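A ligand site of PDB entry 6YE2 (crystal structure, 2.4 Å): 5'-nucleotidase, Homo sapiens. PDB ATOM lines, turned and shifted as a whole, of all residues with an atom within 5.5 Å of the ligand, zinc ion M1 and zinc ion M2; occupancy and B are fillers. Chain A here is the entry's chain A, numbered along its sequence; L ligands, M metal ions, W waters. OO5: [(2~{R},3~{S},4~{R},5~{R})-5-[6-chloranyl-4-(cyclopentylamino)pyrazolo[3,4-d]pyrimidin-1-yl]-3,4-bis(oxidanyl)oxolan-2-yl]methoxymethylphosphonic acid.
Residues that only touch zinc ion M2: His 93 (3.96 Å). Within 4 Å of zinc ion M2: Asp 11, Asp 60, Asn 92, His 93, His 195 and His 218.
Zinc ion M1 is bound by OD1 of Asp 11, O4 of the ligand, NE2 of His 13, water W2 and OD2 of Asp 60.
Three residues have an atom within 4 Å of zinc ion M1: Asp 11, His 13 and Asp 60. The nearest printed residue that does not touch zinc ion M1 is Asn 220 (4.1 Å).
The backbone carbonyl oxygen (O) of Gly 367 lies close to an oxygen (O7) of the ligand. OD1 of Asp 96 touches C15 of the ligand, 3.3 Å away. O of Leu 159 touches C4 of the ligand, at 3.1 Å. Ser 160 touches the ligand (CA to C6, 3.6 Å). Asn 161 touches the ligand. Gly 368 touches the ligand. Phe 392 touches the ligand. Phe 475 touches the ligand (CD1 to N5, 3.5 Å). Hydrophobic or aromatic side chains that line the ligand: His 93, Leu 159, His 218, Phe 392 and Phe 475. Of the 28 residues printed, 19 come within 4 Å of the ligand. The nearest printed residue that does not touch the ligand is His 195 (4.03 Å).
The backbone carbonyl oxygen of Gly 422 is in hydrogen-bond range of the backbone NH of Gly 366, at 3.4 Å. ND2 of Asn 365 lies close to N of Gly 368, at 3.1 Å. The side-chain hydroxyl (OG) of Ser 160 sits at hydrogen-bond distance from the side-chain carboxylate (OD1) of Asp 96 (2.7 Å). The guanidinium group (NH2) of Arg 370 lies within hydrogen-bond range of the backbone carbonyl oxygen (O) of Gly 367, 3.0 Å away. N of Gly 367 is in hydrogen-bond range of O of Gly 422, 3.0 Å away. N of His 218 sits at hydrogen-bond distance from OD2 of Asp 11 (2.7 Å). NH2 of Arg 329 sits at hydrogen-bond distance from O of Gly 367 (3.4 Å). O of Asp 96 sits at hydrogen-bond distance from ND2 of Asn 161, at 2.9 Å.
A ring nitrogen (NE2) of His 93 sits at hydrogen-bond distance from an oxygen (O6) of the ligand (2.8 Å). OD2 of Asp 481 sits at hydrogen-bond distance from O2 of the ligand (2.7 Å). NH1 of Arg 370 is in salt-bridge range of O6 of the ligand, 2.7 Å away. O of Gly 422 sits at hydrogen-bond distance from O2 of the ligand, at 3.3 Å. ND2 of Asn 365 sits at hydrogen-bond distance from O2 of the ligand (2.9 Å). An oxygen (O3) of the ligand sits at hydrogen-bond distance from the guanidinium group of Arg 329 (2.9 Å).
Zinc ion M2 is bound by O5 of the ligand, OD1 of Asn 92, NE2 of His 195, ND1 of His 218 and OD2 of Asp 60. Slightly farther from zinc ion M2 lies an oxygen (O4) of the ligand (2.7 Å).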
ATOM      1  N   ASP A  11       7.459   3.780   0.447  1.00  0.00           N
ATOM      2  CA  ASP A  11       6.858   5.005   0.925  1.00  0.00           C
ATOM      3  C   ASP A  11       7.093   5.261   2.400  1.00  0.00           C
ATOM      4  O   ASP A  11       6.155   5.630   3.106  1.00  0.00           O
ATOM      5  CB  ASP A  11       5.360   5.020   0.584  1.00  0.00           C
ATOM      6  CG  ASP A  11       5.148   4.965  -0.908  1.00  0.00           C
ATOM      7  OD1 ASP A  11       5.194   6.027  -1.542  1.00  0.00           O
ATOM      8  OD2 ASP A  11       4.988   3.868  -1.428  1.00  0.00           O
ATOM      9  N   HIS A  13       8.805   7.731   3.707  1.00  0.00           N
ATOM     10  CA  HIS A  13       8.604   9.160   3.827  1.00  0.00           C
ATOM     11  C   HIS A  13       9.129   9.812   5.112  1.00  0.00           C
ATOM     12  O   HIS A  13       8.386  10.456   5.864  1.00  0.00           O
ATOM     13  CB  HIS A  13       7.138   9.503   3.620  1.00  0.00           C
ATOM     14  CG  HIS A  13       6.732   9.409   2.194  1.00  0.00           C
ATOM     15  ND1 HIS A  13       7.430  10.095   1.212  1.00  0.00           N
ATOM     16  CD2 HIS A  13       5.741   8.705   1.617  1.00  0.00           C
ATOM     17  CE1 HIS A  13       6.855   9.776   0.071  1.00  0.00           C
ATOM     18  NE2 HIS A  13       5.835   8.938   0.263  1.00  0.00           N
ATOM     19  N   ASP A  60      10.364   6.376  -2.414  1.00  0.00           N
ATOM     20  CA  ASP A  60       9.718   7.360  -1.569  1.00  0.00           C
ATOM     21  C   ASP A  60      10.192   7.307  -0.126  1.00  0.00           C
ATOM     22  O   ASP A  60       9.421   7.418   0.833  1.00  0.00           O
ATOM     23  CB  ASP A  60       8.194   7.292  -1.692  1.00  0.00           C
ATOM     24  CG  ASP A  60       7.607   8.142  -2.807  1.00  0.00           C
ATOM     25  OD1 ASP A  60       8.407   8.709  -3.627  1.00  0.00           O
ATOM     26  OD2 ASP A  60       6.355   8.241  -2.879  1.00  0.00           O
ATOM     27  N   GLN A  63      11.096  12.939   1.605  1.00  0.00           N
ATOM     28  CA  GLN A  63      10.008  13.879   1.932  1.00  0.00           C
ATOM     29  C   GLN A  63       8.968  13.312   2.883  1.00  0.00           C
ATOM     30  O   GLN A  63       8.386  12.274   2.603  1.00  0.00           O
ATOM     31  CB  GLN A  63       9.369  14.384   0.609  1.00  0.00           C
ATOM     32  CG  GLN A  63       8.717  15.761   0.665  1.00  0.00           C
ATOM     33  CD  GLN A  63       9.690  16.921   0.683  1.00  0.00           C
ATOM     34  OE1 GLN A  63      10.050  17.473   1.742  1.00  0.00           O
ATOM     35  NE2 GLN A  63      10.092  17.328  -0.499  1.00  0.00           N
ATOM     36  N   GLY A  91      11.773   6.572  -6.376  1.00  0.00           N
ATOM     37  CA  GLY A  91      10.397   7.018  -6.298  1.00  0.00           C
ATOM     38  C   GLY A  91      10.299   8.415  -6.878  1.00  0.00           C
ATOM     39  O   GLY A  91      11.323   9.037  -7.193  1.00  0.00           O
ATOM     40  N   ASN A  92       9.081   8.905  -7.041  1.00  0.00           N
ATOM     41  CA  ASN A  92       8.902  10.257  -7.566  1.00  0.00           C
ATOM     42  C   ASN A  92       9.472  11.312  -6.574  1.00  0.00           C
ATOM     43  O   ASN A  92      10.105  12.278  -7.021  1.00  0.00           O
ATOM     44  CB  ASN A  92       7.433  10.532  -7.915  1.00  0.00           C
ATOM     45  CG  ASN A  92       6.495  10.276  -6.768  1.00  0.00           C
ATOM     46  OD1 ASN A  92       6.205   9.135  -6.413  1.00  0.00           O
ATOM     47  ND2 ASN A  92       6.031  11.337  -6.152  1.00  0.00           N
ATOM     48  N   HIS A  93       9.304  11.097  -5.235  1.00  0.00           N
ATOM     49  CA  HIS A  93       9.765  12.047  -4.206  1.00  0.00           C
ATOM     50  C   HIS A  93      11.281  12.167  -4.106  1.00  0.00           C
ATOM     51  O   HIS A  93      11.748  13.172  -3.576  1.00  0.00           O
ATOM     52  CB  HIS A  93       9.128  11.770  -2.837  1.00  0.00           C
ATOM     53  CG  HIS A  93       7.679  12.152  -2.829  1.00  0.00           C
ATOM     54  ND1 HIS A  93       7.294  13.457  -2.648  1.00  0.00           N
ATOM     55  CD2 HIS A  93       6.596  11.410  -3.104  1.00  0.00           C
ATOM     56  CE1 HIS A  93       5.980  13.455  -2.770  1.00  0.00           C
ATOM     57  NE2 HIS A  93       5.529  12.250  -3.057  1.00  0.00           N
ATOM     58  N   ASP A  96      12.288  15.504  -5.548  1.00  0.00           N
ATOM     59  CA  ASP A  96      11.731  16.725  -4.927  1.00  0.00           C
ATOM     60  C   ASP A  96      12.719  17.873  -4.781  1.00  0.00           C
ATOM     61  O   ASP A  96      12.313  19.043  -4.830  1.00  0.00           O
ATOM     62  CB  ASP A  96      11.076  16.409  -3.573  1.00  0.00           C
ATOM     63  CG  ASP A  96       9.762  15.666  -3.668  1.00  0.00           C
ATOM     64  OD1 ASP A  96       9.378  15.241  -4.786  1.00  0.00           O
ATOM     65  OD2 ASP A  96       9.112  15.502  -2.633  1.00  0.00           O
ATOM     66  N   LEU A 159       4.727  15.339 -10.751  1.00  0.00           N
ATOM     67  CA  LEU A 159       4.628  15.148  -9.294  1.00  0.00           C
ATOM     68  C   LEU A 159       5.836  15.720  -8.582  1.00  0.00           C
ATOM     69  O   LEU A 159       5.760  15.969  -7.370  1.00  0.00           O
ATOM     70  CB  LEU A 159       4.516  13.649  -8.934  1.00  0.00           C
ATOM     71  CG  LEU A 159       3.271  12.919  -9.376  1.00  0.00           C
ATOM     72  CD1 LEU A 159       3.462  11.413  -9.304  1.00  0.00           C
ATOM     73  CD2 LEU A 159       2.064  13.394  -8.648  1.00  0.00           C
ATOM     74  N   SER A 160       6.941  15.915  -9.303  1.00  0.00           N
ATOM     75  CA  SER A 160       8.194  16.318  -8.698  1.00  0.00           C
ATOM     76  C   SER A 160       8.991  17.272  -9.554  1.00  0.00           C
ATOM     77  O   SER A 160       8.466  17.819 -10.522  1.00  0.00           O
ATOM     78  CB  SER A 160       9.023  15.066  -8.393  1.00  0.00           C
ATOM     79  OG  SER A 160      10.021  15.340  -7.425  1.00  0.00           O
ATOM     80  N   ASN A 161      10.276  17.458  -9.205  1.00  0.00           N
ATOM     81  CA  ASN A 161      11.204  18.333  -9.904  1.00  0.00           C
ATOM     82  C   ASN A 161      12.354  17.513 -10.537  1.00  0.00           C
ATOM     83  O   ASN A 161      13.513  17.813 -10.231  1.00  0.00           O
ATOM     84  CB  ASN A 161      11.749  19.413  -8.943  1.00  0.00           C
ATOM     85  CG  ASN A 161      10.719  20.259  -8.244  1.00  0.00           C
ATOM     86  OD1 ASN A 161       9.824  20.875  -8.856  1.00  0.00           O
ATOM     87  ND2 ASN A 161      10.853  20.350  -6.937  1.00  0.00           N
ATOM     88  N   HIS A 195       8.165   2.068  -8.414  1.00  0.00           N
ATOM     89  CA  HIS A 195       7.313   3.099  -7.828  1.00  0.00           C
ATOM     90  C   HIS A 195       6.320   3.754  -8.783  1.00  0.00           C
ATOM     91  O   HIS A 195       6.497   4.916  -9.143  1.00  0.00           O
ATOM     92  CB  HIS A 195       8.216   4.146  -7.186  1.00  0.00           C
ATOM     93  CG  HIS A 195       7.509   4.956  -6.159  1.00  0.00           C
ATOM     94  ND1 HIS A 195       7.460   4.555  -4.852  1.00  0.00           N
ATOM     95  CD2 HIS A 195       6.845   6.131  -6.294  1.00  0.00           C
ATOM     96  CE1 HIS A 195       6.760   5.484  -4.233  1.00  0.00           C
ATOM     97  NE2 HIS A 195       6.380   6.462  -5.068  1.00  0.00           N
ATOM     98  N   HIS A 218       4.018   3.728  -3.954  1.00  0.00           N
ATOM     99  CA  HIS A 218       3.305   4.890  -4.502  1.00  0.00           C
ATOM    100  C   HIS A 218       1.816   4.974  -4.157  1.00  0.00           C
ATOM    101  O   HIS A 218       1.336   6.077  -3.877  1.00  0.00           O
ATOM    102  CB  HIS A 218       3.527   5.003  -6.029  1.00  0.00           C
ATOM    103  CG  HIS A 218       3.068   6.307  -6.615  1.00  0.00           C
ATOM    104  ND1 HIS A 218       3.773   7.486  -6.409  1.00  0.00           N
ATOM    105  CD2 HIS A 218       2.042   6.555  -7.464  1.00  0.00           C
ATOM    106  CE1 HIS A 218       3.142   8.414  -7.109  1.00  0.00           C
ATOM    107  NE2 HIS A 218       2.095   7.903  -7.746  1.00  0.00           N
ATOM    108  N   SER A 219       1.078   3.859  -4.224  1.00  0.00           N
ATOM    109  CA  SER A 219      -0.366   3.858  -3.931  1.00  0.00           C
ATOM    110  C   SER A 219      -0.657   3.582  -2.442  1.00  0.00           C
ATOM    111  O   SER A 219      -1.842   3.602  -2.050  1.00  0.00           O
ATOM    112  CB  SER A 219      -1.073   2.830  -4.803  1.00  0.00           C
ATOM    113  OG  SER A 219      -0.312   1.637  -4.938  1.00  0.00           O
ATOM    114  N   ASN A 220       0.419   3.341  -1.609  1.00  0.00           N
ATOM    115  CA  ASN A 220       0.339   3.049  -0.174  1.00  0.00           C
ATOM    116  C   ASN A 220      -0.615   1.870   0.040  1.00  0.00           C
ATOM    117  O   ASN A 220      -1.463   1.912   0.937  1.00  0.00           O
ATOM    118  CB  ASN A 220      -0.130   4.301   0.611  1.00  0.00           C
ATOM    119  CG  ASN A 220       0.912   5.390   0.745  1.00  0.00           C
ATOM    120  OD1 ASN A 220       1.930   5.388   0.068  1.00  0.00           O
ATOM    121  ND2 ASN A 220       0.676   6.338   1.640  1.00  0.00           N
ATOM    122  N   ARG A 329      -8.330  11.741   0.451  1.00  0.00           N
ATOM    123  CA  ARG A 329      -8.324  11.375  -0.962  1.00  0.00           C
ATOM    124  C   ARG A 329      -9.639  10.678  -1.341  1.00  0.00           C
ATOM    125  O   ARG A 329      -9.825  10.334  -2.514  1.00  0.00           O
ATOM    126  CB  ARG A 329      -7.136  10.458  -1.291  1.00  0.00           C
ATOM    127  CG  ARG A 329      -5.759  11.068  -1.008  1.00  0.00           C
ATOM    128  CD  ARG A 329      -4.667  10.103  -1.394  1.00  0.00           C
ATOM    129  NE  ARG A 329      -3.354  10.643  -1.051  1.00  0.00           N
ATOM    130  CZ  ARG A 329      -2.273  10.541  -1.829  1.00  0.00           C
ATOM    131  NH1 ARG A 329      -2.342   9.950  -3.008  1.00  0.00           N
ATOM    132  NH2 ARG A 329      -1.117  11.064  -1.431  1.00  0.00           N
ATOM    133  N   ASN A 365      -5.614  19.731  -3.333  1.00  0.00           N
ATOM    134  CA  ASN A 365      -5.423  18.298  -3.612  1.00  0.00           C
ATOM    135  C   ASN A 365      -5.181  17.559  -2.299  1.00  0.00           C
ATOM    136  O   ASN A 365      -4.223  17.865  -1.587  1.00  0.00           O
ATOM    137  CB  ASN A 365      -4.280  18.095  -4.610  1.00  0.00           C
ATOM    138  CG  ASN A 365      -2.958  18.635  -4.099  1.00  0.00           C
ATOM    139  OD1 ASN A 365      -2.788  19.821  -3.824  1.00  0.00           O
ATOM    140  ND2 ASN A 365      -2.008  17.745  -3.894  1.00  0.00           N
ATOM    141  N   GLY A 366      -6.099  16.668  -1.935  1.00  0.00           N
ATOM    142  CA  GLY A 366      -6.034  15.870  -0.714  1.00  0.00           C
ATOM    143  C   GLY A 366      -4.713  15.135  -0.560  1.00  0.00           C
ATOM    144  O   GLY A 366      -4.231  14.967   0.555  1.00  0.00           O
ATOM    145  N   GLY A 367      -4.109  14.771  -1.685  1.00  0.00           N
ATOM    146  CA  GLY A 367      -2.814  14.104  -1.705  1.00  0.00           C
ATOM    147  C   GLY A 367      -1.669  14.957  -1.175  1.00  0.00           C
ATOM    148  O   GLY A 367      -0.623  14.412  -0.840  1.00  0.00           O
ATOM    149  N   GLY A 368      -1.873  16.273  -1.114  1.00  0.00           N
ATOM    150  CA  GLY A 368      -0.902  17.230  -0.589  1.00  0.00           C
ATOM    151  C   GLY A 368      -0.942  17.352   0.922  1.00  0.00           C
ATOM    152  O   GLY A 368      -0.196  18.150   1.499  1.00  0.00           O
ATOM    153  N   ARG A 370      -0.253  15.305   4.147  1.00  0.00           N
ATOM    154  CA  ARG A 370       0.710  14.252   4.342  1.00  0.00           C
ATOM    155  C   ARG A 370       0.705  13.566   5.704  1.00  0.00           C
ATOM    156  O   ARG A 370       1.382  12.537   5.849  1.00  0.00           O
ATOM    157  CB  ARG A 370       2.101  14.814   4.005  1.00  0.00           C
ATOM    158  CG  ARG A 370       2.148  15.449   2.619  1.00  0.00           C
ATOM    159  CD  ARG A 370       1.719  14.536   1.490  1.00  0.00           C
ATOM    160  NE  ARG A 370       2.609  13.393   1.343  1.00  0.00           N
ATOM    161  CZ  ARG A 370       2.670  12.607   0.283  1.00  0.00           C
ATOM    162  NH1 ARG A 370       3.502  11.578   0.257  1.00  0.00           N
ATOM    163  NH2 ARG A 370       1.920  12.850  -0.779  1.00  0.00           N
ATOM    164  N   PHE A 392       6.058  19.998   1.649  1.00  0.00           N
ATOM    165  CA  PHE A 392       6.519  20.316   0.300  1.00  0.00           C
ATOM    166  C   PHE A 392       7.089  21.721   0.083  1.00  0.00           C
ATOM    167  O   PHE A 392       7.695  21.927  -0.956  1.00  0.00           O
ATOM    168  CB  PHE A 392       5.426  20.020  -0.713  1.00  0.00           C
ATOM    169  CG  PHE A 392       4.970  18.567  -0.682  1.00  0.00           C
ATOM    170  CD1 PHE A 392       5.887  17.529  -0.695  1.00  0.00           C
ATOM    171  CD2 PHE A 392       3.619  18.249  -0.628  1.00  0.00           C
ATOM    172  CE1 PHE A 392       5.457  16.198  -0.686  1.00  0.00           C
ATOM    173  CE2 PHE A 392       3.201  16.920  -0.637  1.00  0.00           C
ATOM    174  CZ  PHE A 392       4.124  15.904  -0.661  1.00  0.00           C
ATOM    175  N   THR A 421      -5.677   8.151  -5.513  1.00  0.00           N
ATOM    176  CA  THR A 421      -4.894   9.175  -6.185  1.00  0.00           C
ATOM    177  C   THR A 421      -5.123  10.509  -5.475  1.00  0.00           C
ATOM    178  O   THR A 421      -6.190  10.759  -4.887  1.00  0.00           O
ATOM    179  CB  THR A 421      -5.161   9.182  -7.686  1.00  0.00           C
ATOM    180  OG1 THR A 421      -6.563   9.324  -7.894  1.00  0.00           O
ATOM    181  CG2 THR A 421      -4.637   7.919  -8.376  1.00  0.00           C
ATOM    182  N   GLY A 422      -4.081  11.328  -5.481  1.00  0.00           N
ATOM    183  CA  GLY A 422      -4.013  12.589  -4.766  1.00  0.00           C
ATOM    184  C   GLY A 422      -4.838  13.735  -5.266  1.00  0.00           C
ATOM    185  O   GLY A 422      -5.017  14.710  -4.515  1.00  0.00           O
ATOM    186  N   GLU A 423      -5.355  13.666  -6.505  1.00  0.00           N
ATOM    187  CA  GLU A 423      -6.079  14.780  -7.129  1.00  0.00           C
ATOM    188  C   GLU A 423      -7.433  15.126  -6.483  1.00  0.00           C
ATOM    189  O   GLU A 423      -7.872  16.241  -6.667  1.00  0.00           O
ATOM    190  CB  GLU A 423      -6.210  14.616  -8.661  1.00  0.00           C
ATOM    191  CG  GLU A 423      -7.287  13.670  -9.169  1.00  0.00           C
ATOM    192  CD  GLU A 423      -6.797  12.279  -9.465  1.00  0.00           C
ATOM    193  OE1 GLU A 423      -7.637  11.394  -9.767  1.00  0.00           O
ATOM    194  OE2 GLU A 423      -5.568  12.049  -9.387  1.00  0.00           O
ATOM    195  N   PRO A 473      -2.926  25.637  -3.745  1.00  0.00           N
ATOM    196  CA  PRO A 473      -1.456  25.528  -3.663  1.00  0.00           C
ATOM    197  C   PRO A 473      -0.809  25.773  -5.034  1.00  0.00           C
ATOM    198  O   PRO A 473      -1.439  25.488  -6.058  1.00  0.00           O
ATOM    199  CB  PRO A 473      -1.231  24.111  -3.156  1.00  0.00           C
ATOM    200  CG  PRO A 473      -2.466  23.363  -3.533  1.00  0.00           C
ATOM    201  CD  PRO A 473      -3.573  24.342  -3.475  1.00  0.00           C
ATOM    202  N   PHE A 475       1.391  24.135  -6.603  1.00  0.00           N
ATOM    203  CA  PHE A 475       1.405  22.845  -7.281  1.00  0.00           C
ATOM    204  C   PHE A 475       0.243  22.700  -8.274  1.00  0.00           C
ATOM    205  O   PHE A 475       0.456  22.286  -9.406  1.00  0.00           O
ATOM    206  CB  PHE A 475       1.393  21.712  -6.225  1.00  0.00           C
ATOM    207  CG  PHE A 475       1.253  20.311  -6.778  1.00  0.00           C
ATOM    208  CD1 PHE A 475       2.258  19.729  -7.536  1.00  0.00           C
ATOM    209  CD2 PHE A 475       0.105  19.551  -6.530  1.00  0.00           C
ATOM    210  CE1 PHE A 475       2.141  18.432  -8.028  1.00  0.00           C
ATOM    211  CE2 PHE A 475      -0.019  18.249  -7.026  1.00  0.00           C
ATOM    212  CZ  PHE A 475       1.001  17.702  -7.762  1.00  0.00           C
ATOM    213  N   ASP A 481      -0.861  17.571 -10.720  1.00  0.00           N
ATOM    214  CA  ASP A 481      -1.853  16.524 -10.450  1.00  0.00           C
ATOM    215  C   ASP A 481      -2.836  16.274 -11.601  1.00  0.00           C
ATOM    216  O   ASP A 481      -3.917  15.750 -11.349  1.00  0.00           O
ATOM    217  CB  ASP A 481      -2.614  16.786  -9.126  1.00  0.00           C
ATOM    218  CG  ASP A 481      -2.420  15.719  -8.083  1.00  0.00           C
ATOM    219  OD1 ASP A 481      -1.964  14.598  -8.450  1.00  0.00           O
ATOM    220  OD2 ASP A 481      -2.741  15.987  -6.910  1.00  0.00           O
HETATM  221  N1  OO5 L   1       2.873  19.502  -3.755  1.00  0.00           N
HETATM  222  N2  OO5 L   1       1.198  17.850  -3.281  1.00  0.00           N
HETATM  223  C1  OO5 L   1       1.976  16.986  -3.934  1.00  0.00           C
HETATM  224  C2  OO5 L   1       3.191  17.268  -4.537  1.00  0.00           C
HETATM  225  C3  OO5 L   1       3.603  18.614  -4.438  1.00  0.00           C
HETATM  226  C4  OO5 L   1       3.622  16.026  -5.082  1.00  0.00           C
HETATM  227  C5  OO5 L   1       5.898  19.562  -4.547  1.00  0.00           C
HETATM  228  C6  OO5 L   1       7.348  18.860  -6.264  1.00  0.00           C
HETATM  229  O1  OO5 L   1      -1.043  12.913  -6.465  1.00  0.00           O
HETATM  230  C7  OO5 L   1      -0.056  13.505  -5.630  1.00  0.00           C
HETATM  231  C8  OO5 L   1      -0.419  14.872  -5.067  1.00  0.00           C
HETATM  232  O2  OO5 L   1      -1.764  14.973  -4.639  1.00  0.00           O
HETATM  233  C9  OO5 L   1       0.188  12.695  -4.364  1.00  0.00           C
HETATM  234  C10 OO5 L   1       1.089  11.492  -4.563  1.00  0.00           C
HETATM  235  O3  OO5 L   1       0.810  10.539  -3.564  1.00  0.00           O
HETATM  236  C11 OO5 L   1       1.559   9.339  -3.718  1.00  0.00           C
HETATM  237  P1  OO5 L   1       3.308   9.615  -3.363  1.00  0.00           P
HETATM  238  O4  OO5 L   1       3.757   8.328  -2.642  1.00  0.00           O
HETATM  239  O5  OO5 L   1       4.177   9.873  -4.557  1.00  0.00           O
HETATM  240  O6  OO5 L   1       3.336  10.743  -2.319  1.00  0.00           O
HETATM  241  O7  OO5 L   1       0.758  13.626  -3.425  1.00  0.00           O
HETATM  242  C12 OO5 L   1       0.504  14.957  -3.845  1.00  0.00           C
HETATM  243  N3  OO5 L   1       1.733  15.662  -4.129  1.00  0.00           N
HETATM  244  N4  OO5 L   1       2.756  15.067  -4.818  1.00  0.00           N
HETATM  245  C13 OO5 L   1       1.727  19.071  -3.253  1.00  0.00           C
HETATM  246 CL1  OO5 L   1       0.710  20.298  -2.564  1.00  0.00          CL
HETATM  247  N5  OO5 L   1       4.670  19.039  -5.123  1.00  0.00           N
HETATM  248  C14 OO5 L   1       6.792  20.093  -5.637  1.00  0.00           C
HETATM  249  C15 OO5 L   1       7.427  17.844  -5.116  1.00  0.00           C
HETATM  250  C16 OO5 L   1       6.731  18.455  -3.941  1.00  0.00           C
HETATM  251 ZN    ZN M   1       4.934   7.880  -1.162  1.00  0.00          ZN
HETATM  252 ZN    ZN M   2       5.210   8.163  -4.892  1.00  0.00          ZN
HETATM  253  O   HOH W   1       5.798  22.811  -3.834  1.00  0.00           O
HETATM  254  O   HOH W   2       3.262   7.656  -0.074  1.00  0.00           O
HETATM  255  O   HOH W   3      -0.324  21.936  -0.394  1.00  0.00           O
